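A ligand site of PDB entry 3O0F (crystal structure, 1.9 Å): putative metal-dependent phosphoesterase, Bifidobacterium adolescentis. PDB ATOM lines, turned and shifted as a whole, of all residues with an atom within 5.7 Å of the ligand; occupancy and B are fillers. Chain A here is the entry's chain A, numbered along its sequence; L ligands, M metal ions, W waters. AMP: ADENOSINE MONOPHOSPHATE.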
ATOM      1  N   ASP A  25      -9.413   7.051  26.189  1.00  0.00           N
ATOM      2  CA  ASP A  25      -9.969   6.520  24.960  1.00  0.00           C
ATOM      3  C   ASP A  25     -10.506   5.072  25.016  1.00  0.00           C
ATOM      4  O   ASP A  25     -10.782   4.475  23.976  1.00  0.00           O
ATOM      5  CB  ASP A  25      -8.997   6.705  23.791  1.00  0.00           C
ATOM      6  CG  ASP A  25      -7.637   6.035  23.990  1.00  0.00           C
ATOM      7  OD1 ASP A  25      -7.308   5.534  25.107  1.00  0.00           O
ATOM      8  OD2 ASP A  25      -6.867   6.012  22.976  1.00  0.00           O
ATOM      9  N   HIS A  50      -4.363   8.035  29.140  1.00  0.00           N
ATOM     10  CA  HIS A  50      -3.510   9.057  28.499  1.00  0.00           C
ATOM     11  C   HIS A  50      -3.531  10.355  29.299  1.00  0.00           C
ATOM     12  O   HIS A  50      -4.594  10.888  29.563  1.00  0.00           O
ATOM     13  CB  HIS A  50      -4.044   9.353  27.094  1.00  0.00           C
ATOM     14  CG  HIS A  50      -3.962   8.197  26.170  1.00  0.00           C
ATOM     15  ND1 HIS A  50      -2.796   7.854  25.518  1.00  0.00           N
ATOM     16  CD2 HIS A  50      -4.894   7.289  25.783  1.00  0.00           C
ATOM     17  CE1 HIS A  50      -3.009   6.782  24.781  1.00  0.00           C
ATOM     18  NE2 HIS A  50      -4.268   6.435  24.908  1.00  0.00           N
ATOM     19  N   THR A  77       1.977  11.092  26.732  1.00  0.00           N
ATOM     20  CA  THR A  77       2.304  11.413  25.346  1.00  0.00           C
ATOM     21  C   THR A  77       3.614  12.229  25.297  1.00  0.00           C
ATOM     22  O   THR A  77       3.745  13.216  26.004  1.00  0.00           O
ATOM     23  CB  THR A  77       1.140  12.295  24.741  1.00  0.00           C
ATOM     24  OG1 THR A  77      -0.124  11.710  25.062  1.00  0.00           O
ATOM     25  CG2 THR A  77       1.245  12.444  23.209  1.00  0.00           C
ATOM     26  N   HIS A  86       5.309   6.971  23.606  1.00  0.00           N
ATOM     27  CA  HIS A  86       4.412   6.887  24.729  1.00  0.00           C
ATOM     28  C   HIS A  86       5.168   6.267  25.908  1.00  0.00           C
ATOM     29  O   HIS A  86       5.863   5.254  25.758  1.00  0.00           O
ATOM     30  CB  HIS A  86       3.187   6.049  24.309  1.00  0.00           C
ATOM     31  CG  HIS A  86       2.260   6.783  23.384  1.00  0.00           C
ATOM     32  ND1 HIS A  86       0.976   6.349  23.106  1.00  0.00           N
ATOM     33  CD2 HIS A  86       2.408   7.953  22.704  1.00  0.00           C
ATOM     34  CE1 HIS A  86       0.397   7.202  22.281  1.00  0.00           C
ATOM     35  NE2 HIS A  86       1.238   8.180  22.026  1.00  0.00           N
ATOM     36  N   ARG A 110      -4.056  19.015  23.467  1.00  0.00           N
ATOM     37  CA  ARG A 110      -4.980  17.997  22.877  1.00  0.00           C
ATOM     38  C   ARG A 110      -6.408  18.519  22.533  1.00  0.00           C
ATOM     39  O   ARG A 110      -6.915  18.296  21.445  1.00  0.00           O
ATOM     40  CB  ARG A 110      -5.144  16.804  23.808  1.00  0.00           C
ATOM     41  CG  ARG A 110      -3.984  15.822  23.798  1.00  0.00           C
ATOM     42  CD  ARG A 110      -4.255  14.668  24.794  1.00  0.00           C
ATOM     43  NE  ARG A 110      -3.383  13.528  24.475  1.00  0.00           N
ATOM     44  CZ  ARG A 110      -3.534  12.729  23.410  1.00  0.00           C
ATOM     45  NH1 ARG A 110      -4.527  12.897  22.562  1.00  0.00           N
ATOM     46  NH2 ARG A 110      -2.673  11.742  23.204  1.00  0.00           N
ATOM     47  N   ARG A 113      -6.077  21.102  19.605  1.00  0.00           N
ATOM     48  CA  ARG A 113      -5.739  20.388  18.401  1.00  0.00           C
ATOM     49  C   ARG A 113      -6.925  19.599  17.829  1.00  0.00           C
ATOM     50  O   ARG A 113      -7.130  19.513  16.607  1.00  0.00           O
ATOM     51  CB  ARG A 113      -4.639  19.382  18.780  1.00  0.00           C
ATOM     52  CG  ARG A 113      -3.764  18.852  17.699  1.00  0.00           C
ATOM     53  CD  ARG A 113      -4.212  17.543  17.055  1.00  0.00           C
ATOM     54  NE  ARG A 113      -4.735  16.523  17.937  1.00  0.00           N
ATOM     55  CZ  ARG A 113      -4.445  15.219  17.883  1.00  0.00           C
ATOM     56  NH1 ARG A 113      -3.593  14.697  17.003  1.00  0.00           N
ATOM     57  NH2 ARG A 113      -5.010  14.417  18.755  1.00  0.00           N
ATOM     58  N   THR A 114      -7.662  18.952  18.730  1.00  0.00           N
ATOM     59  CA  THR A 114      -8.690  18.011  18.343  1.00  0.00           C
ATOM     60  C   THR A 114      -9.886  18.809  17.807  1.00  0.00           C
ATOM     61  O   THR A 114     -10.498  18.422  16.833  1.00  0.00           O
ATOM     62  CB  THR A 114      -9.011  17.029  19.499  1.00  0.00           C
ATOM     63  OG1 THR A 114      -7.817  16.262  19.815  1.00  0.00           O
ATOM     64  CG2 THR A 114     -10.117  16.036  19.121  1.00  0.00           C
ATOM     65  N   ILE A 144      -9.007  13.950  25.714  1.00  0.00           N
ATOM     66  CA  ILE A 144      -9.557  13.830  24.381  1.00  0.00           C
ATOM     67  C   ILE A 144      -8.459  13.613  23.327  1.00  0.00           C
ATOM     68  O   ILE A 144      -7.334  14.048  23.478  1.00  0.00           O
ATOM     69  CB  ILE A 144     -10.287  15.116  24.005  1.00  0.00           C
ATOM     70  CG1 ILE A 144     -11.330  14.882  22.906  1.00  0.00           C
ATOM     71  CG2 ILE A 144      -9.250  16.176  23.571  1.00  0.00           C
ATOM     72  CD1 ILE A 144     -12.309  16.065  22.699  1.00  0.00           C
ATOM     73  N   GLY A 145      -8.811  12.963  22.229  1.00  0.00           N
ATOM     74  CA  GLY A 145      -7.890  12.854  21.116  1.00  0.00           C
ATOM     75  C   GLY A 145      -8.587  12.324  19.894  1.00  0.00           C
ATOM     76  O   GLY A 145      -9.810  12.377  19.797  1.00  0.00           O
ATOM     77  N   ARG A 146      -7.806  11.791  18.955  1.00  0.00           N
ATOM     78  CA  ARG A 146      -8.377  11.221  17.714  1.00  0.00           C
ATOM     79  C   ARG A 146      -9.379  10.091  17.900  1.00  0.00           C
ATOM     80  O   ARG A 146     -10.328   9.997  17.107  1.00  0.00           O
ATOM     81  CB  ARG A 146      -7.261  10.854  16.726  1.00  0.00           C
ATOM     82  CG  ARG A 146      -6.622  12.080  16.068  1.00  0.00           C
ATOM     83  CD  ARG A 146      -5.175  11.848  15.784  1.00  0.00           C
ATOM     84  NE  ARG A 146      -4.946  10.806  14.815  1.00  0.00           N
ATOM     85  CZ  ARG A 146      -3.966   9.912  14.836  1.00  0.00           C
ATOM     86  NH1 ARG A 146      -3.082   9.852  15.815  1.00  0.00           N
ATOM     87  NH2 ARG A 146      -3.888   9.022  13.852  1.00  0.00           N
ATOM     88  N   PRO A 147      -9.210   9.211  18.908  1.00  0.00           N
ATOM     89  CA  PRO A 147     -10.228   8.178  19.055  1.00  0.00           C
ATOM     90  C   PRO A 147     -11.660   8.658  19.208  1.00  0.00           C
ATOM     91  O   PRO A 147     -12.560   7.982  18.731  1.00  0.00           O
ATOM     92  CB  PRO A 147      -9.793   7.431  20.318  1.00  0.00           C
ATOM     93  CG  PRO A 147      -8.335   7.547  20.302  1.00  0.00           C
ATOM     94  CD  PRO A 147      -8.077   8.964  19.836  1.00  0.00           C
ATOM     95  N   ARG A 162     -13.969   1.954  14.706  1.00  0.00           N
ATOM     96  CA  ARG A 162     -13.016   3.007  15.028  1.00  0.00           C
ATOM     97  C   ARG A 162     -11.705   2.832  14.279  1.00  0.00           C
ATOM     98  O   ARG A 162     -11.144   3.800  13.761  1.00  0.00           O
ATOM     99  CB  ARG A 162     -12.774   3.031  16.529  1.00  0.00           C
ATOM    100  CG  ARG A 162     -11.954   4.165  17.008  1.00  0.00           C
ATOM    101  CD  ARG A 162     -11.393   3.842  18.392  1.00  0.00           C
ATOM    102  NE  ARG A 162     -12.298   4.146  19.491  1.00  0.00           N
ATOM    103  CZ  ARG A 162     -11.899   4.190  20.770  1.00  0.00           C
ATOM    104  NH1 ARG A 162     -10.637   3.929  21.088  1.00  0.00           N
ATOM    105  NH2 ARG A 162     -12.749   4.511  21.723  1.00  0.00           N
ATOM    106  N   SER A 163     -11.223   1.605  14.208  1.00  0.00           N
ATOM    107  CA  SER A 163     -10.015   1.258  13.409  1.00  0.00           C
ATOM    108  C   SER A 163     -10.109   1.587  11.883  1.00  0.00           C
ATOM    109  O   SER A 163      -9.107   1.908  11.252  1.00  0.00           O
ATOM    110  CB  SER A 163      -9.672  -0.228  13.606  1.00  0.00           C
ATOM    111  OG  SER A 163      -9.565  -0.544  14.989  1.00  0.00           O
ATOM    112  N   PHE A 166      -9.368   5.342  11.495  1.00  0.00           N
ATOM    113  CA  PHE A 166      -7.900   5.540  11.593  1.00  0.00           C
ATOM    114  C   PHE A 166      -7.138   5.129  10.320  1.00  0.00           C
ATOM    115  O   PHE A 166      -6.105   5.718   9.987  1.00  0.00           O
ATOM    116  CB  PHE A 166      -7.344   4.790  12.818  1.00  0.00           C
ATOM    117  CG  PHE A 166      -7.388   5.592  14.072  1.00  0.00           C
ATOM    118  CD1 PHE A 166      -6.396   6.543  14.321  1.00  0.00           C
ATOM    119  CD2 PHE A 166      -8.403   5.429  14.994  1.00  0.00           C
ATOM    120  CE1 PHE A 166      -6.405   7.298  15.474  1.00  0.00           C
ATOM    121  CE2 PHE A 166      -8.431   6.186  16.147  1.00  0.00           C
ATOM    122  CZ  PHE A 166      -7.440   7.133  16.387  1.00  0.00           C
ATOM    123  N   TYR A 177      -5.128  15.539   9.595  1.00  0.00           N
ATOM    124  CA  TYR A 177      -4.279  15.317  10.774  1.00  0.00           C
ATOM    125  C   TYR A 177      -3.513  16.565  11.218  1.00  0.00           C
ATOM    126  O   TYR A 177      -2.914  17.256  10.403  1.00  0.00           O
ATOM    127  CB  TYR A 177      -3.295  14.190  10.488  1.00  0.00           C
ATOM    128  CG  TYR A 177      -2.395  13.889  11.661  1.00  0.00           C
ATOM    129  CD1 TYR A 177      -2.918  13.281  12.801  1.00  0.00           C
ATOM    130  CD2 TYR A 177      -1.022  14.191  11.630  1.00  0.00           C
ATOM    131  CE1 TYR A 177      -2.127  12.988  13.874  1.00  0.00           C
ATOM    132  CE2 TYR A 177      -0.211  13.900  12.735  1.00  0.00           C
ATOM    133  CZ  TYR A 177      -0.783  13.299  13.852  1.00  0.00           C
ATOM    134  OH  TYR A 177      -0.046  12.982  14.974  1.00  0.00           O
ATOM    135  N   THR A 180      -0.181  16.786  18.037  1.00  0.00           N
ATOM    136  CA  THR A 180      -0.331  17.481  19.319  1.00  0.00           C
ATOM    137  C   THR A 180       1.045  17.944  19.826  1.00  0.00           C
ATOM    138  O   THR A 180       1.964  17.128  19.912  1.00  0.00           O
ATOM    139  CB  THR A 180      -0.951  16.592  20.421  1.00  0.00           C
ATOM    140  OG1 THR A 180      -2.215  16.075  19.993  1.00  0.00           O
ATOM    141  CG2 THR A 180      -1.172  17.432  21.677  1.00  0.00           C
ATOM    142  N   HIS A 263      -8.608  -1.225  25.241  1.00  0.00           N
ATOM    143  CA  HIS A 263      -9.449  -0.053  25.201  1.00  0.00           C
ATOM    144  C   HIS A 263     -10.911  -0.499  25.154  1.00  0.00           C
ATOM    145  O   HIS A 263     -11.776   0.214  24.633  1.00  0.00           O
ATOM    146  CB  HIS A 263      -9.139   0.756  23.932  1.00  0.00           C
ATOM    147  CG  HIS A 263      -7.824   1.460  23.931  1.00  0.00           C
ATOM    148  ND1 HIS A 263      -6.599   0.813  23.945  1.00  0.00           N
ATOM    149  CD2 HIS A 263      -7.536   2.778  23.866  1.00  0.00           C
ATOM    150  CE1 HIS A 263      -5.632   1.702  23.899  1.00  0.00           C
ATOM    151  NE2 HIS A 263      -6.177   2.902  23.840  1.00  0.00           N
ATOM    152  N   GLY A 266     -13.029  -0.276  21.905  1.00  0.00           N
ATOM    153  CA  GLY A 266     -12.325   0.660  21.023  1.00  0.00           C
ATOM    154  C   GLY A 266     -11.220   0.068  20.165  1.00  0.00           C
ATOM    155  O   GLY A 266     -10.749   0.683  19.216  1.00  0.00           O
ATOM    156  N   LYS A 267     -10.770  -1.126  20.509  1.00  0.00           N
ATOM    157  CA  LYS A 267      -9.719  -1.803  19.779  1.00  0.00           C
ATOM    158  C   LYS A 267      -9.980  -3.297  19.844  1.00  0.00           C
ATOM    159  O   LYS A 267     -10.690  -3.755  20.701  1.00  0.00           O
ATOM    160  CB  LYS A 267      -8.348  -1.516  20.424  1.00  0.00           C
ATOM    161  CG  LYS A 267      -7.681  -0.187  20.095  1.00  0.00           C
ATOM    162  CD  LYS A 267      -6.249  -0.209  20.606  1.00  0.00           C
ATOM    163  CE  LYS A 267      -5.478   1.082  20.404  1.00  0.00           C
ATOM    164  NZ  LYS A 267      -4.094   0.853  20.902  1.00  0.00           N
ATOM    165  N   PRO A 268      -9.364  -4.077  18.954  1.00  0.00           N
ATOM    166  CA  PRO A 268      -9.448  -5.525  19.065  1.00  0.00           C
ATOM    167  C   PRO A 268      -8.659  -6.123  20.253  1.00  0.00           C
ATOM    168  O   PRO A 268      -8.921  -7.279  20.627  1.00  0.00           O
ATOM    169  CB  PRO A 268      -8.845  -5.998  17.742  1.00  0.00           C
ATOM    170  CG  PRO A 268      -7.889  -4.929  17.387  1.00  0.00           C
ATOM    171  CD  PRO A 268      -8.483  -3.657  17.836  1.00  0.00           C
HETATM  172  P   AMP L   1      -3.896  11.045  19.327  1.00  0.00           P
HETATM  173  O1P AMP L   1      -2.957  10.887  20.479  1.00  0.00           O
HETATM  174  O2P AMP L   1      -5.019  11.972  19.715  1.00  0.00           O
HETATM  175  O3P AMP L   1      -3.223  11.393  17.998  1.00  0.00           O
HETATM  176  O5' AMP L   1      -4.579   9.610  19.113  1.00  0.00           O
HETATM  177  C5' AMP L   1      -3.810   8.517  18.662  1.00  0.00           C
HETATM  178  C4' AMP L   1      -4.109   7.369  19.577  1.00  0.00           C
HETATM  179  O4' AMP L   1      -5.379   6.738  19.277  1.00  0.00           O
HETATM  180  C3' AMP L   1      -3.029   6.301  19.469  1.00  0.00           C
HETATM  181  O3' AMP L   1      -2.226   6.333  20.642  1.00  0.00           O
HETATM  182  C2' AMP L   1      -3.911   5.065  19.466  1.00  0.00           C
HETATM  183  O2' AMP L   1      -3.424   3.727  19.443  1.00  0.00           O
HETATM  184  C1' AMP L   1      -5.317   5.467  19.908  1.00  0.00           C
HETATM  185  N9  AMP L   1      -6.355   4.517  19.458  1.00  0.00           N
HETATM  186  C8  AMP L   1      -7.397   4.133  20.193  1.00  0.00           C
HETATM  187  N7  AMP L   1      -8.167   3.272  19.489  1.00  0.00           N
HETATM  188  C5  AMP L   1      -7.607   3.096  18.283  1.00  0.00           C
HETATM  189  C6  AMP L   1      -7.905   2.310  17.073  1.00  0.00           C
HETATM  190  N6  AMP L   1      -9.011   1.495  17.008  1.00  0.00           N
HETATM  191  N1  AMP L   1      -7.062   2.448  16.038  1.00  0.00           N
HETATM  192  C2  AMP L   1      -5.968   3.240  16.059  1.00  0.00           C
HETATM  193  N3  AMP L   1      -5.635   3.970  17.128  1.00  0.00           N
HETATM  194  C4  AMP L   1      -6.405   3.928  18.255  1.00  0.00           C
HETATM  195 ZN    ZN M   1      -5.343   4.791  24.090  1.00  0.00          ZN
HETATM  196 FE    FE M   2       0.445   3.987  23.292  1.00  0.00          FE
HETATM  197  O   HOH W   1      -0.229  10.182  20.678  1.00  0.00           O
HETATM  198  O   HOH W   2      -0.243   2.776  20.200  1.00  0.00           O
HETATM  199  O   HOH W   3      -3.308   5.105  16.109  1.00  0.00           O
HETATM  200  O   HOH W   4      -0.860  11.530  17.130  1.00  0.00           O
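The guanidinium group of Arg 162 is in hydrogen-bond range of a nitrogen (N7) of the ligand, 3.0 Å away. NH2 of Arg 110 is in salt-bridge range of O1P of the ligand. A nitrogen (N6) of the ligand lies within hydrogen-bond range of the backbone carbonyl oxygen (O) of Gly 266 (2.9 Å). An oxygen (O2') of the ligand lies within hydrogen-bond range of the side-chain amino group (NZ) of Lys 267 (3.3 Å). An oxygen (O2P) of the ligand lies within hydrogen-bond range of the backbone NH (N) of Arg 146, 2.9 Å away. The guanidinium group (NH2) of Arg 113 lies within salt-bridge range of an oxygen (O2P) of the ligand, at 2.6 Å. O3P of the ligand is in salt-bridge range of NH1 of Arg 146 (2.7 Å). N6 of the ligand lies within hydrogen-bond range of OG of Ser 163, 2.9 Å away.
NE of Arg 113 lies close to OG1 of Thr 180, at 3.3 Å. The backbone carbonyl oxygen (O) of Ile 144 sits at hydrogen-bond distance from the guanidinium group (NH1) of Arg 110 (3.2 Å). The backbone carbonyl oxygen (O) of Arg 110 lies within hydrogen-bond range of the side-chain hydroxyl (OG1) of Thr 114, 2.8 Å away. The guanidinium group (NH2) of Arg 110 is in hydrogen-bond range of the side-chain hydroxyl (OG1) of Thr 77, 3.2 Å away. The guanidinium group (NH1) of Arg 162 sits at hydrogen-bond distance from the backbone carbonyl oxygen (O) of Asp 25.
OD2 of Asp 25 touches C8 of the ligand (3.4 Å). CE1 of His 86 touches O3' of the ligand, at 3.2 Å. Gly 145 touches the ligand (CA to O2P, 3.3 Å). CG of Pro 147 touches O4' of the ligand, at 3.2 Å. Phe 166 touches the ligand (CG to C2, 3.4 Å). His 263 touches the ligand. Hydrophobic or aromatic side chains that line the ligand: His 86, Pro 147, Phe 166 and His 263. Within 4 Å of the ligand: Asp 25, His 86, Arg 110, Arg 113, Gly 145, Arg 146, Pro 147, Arg 162, Ser 163, Phe 166, His 263, Gly 266 and Lys 267. Along chain A the residues within 4 Å of the ligand span positions 25 to 267. The nearest printed residue that does not touch the ligand is His 50 (4.2 Å).
Water W4 lies within hydrogen-bond range of an oxygen (O3P) of the ligand (2.5 Å), the side-chain hydroxyl of Tyr 177 (2.7 Å) and the guanidinium group of Arg 146 (3.1 Å). Water W1 lies within hydrogen-bond range of a ring nitrogen (NE2) of His 86 (2.8 Å) and an oxygen (O1P) of the ligand (2.8 Å).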
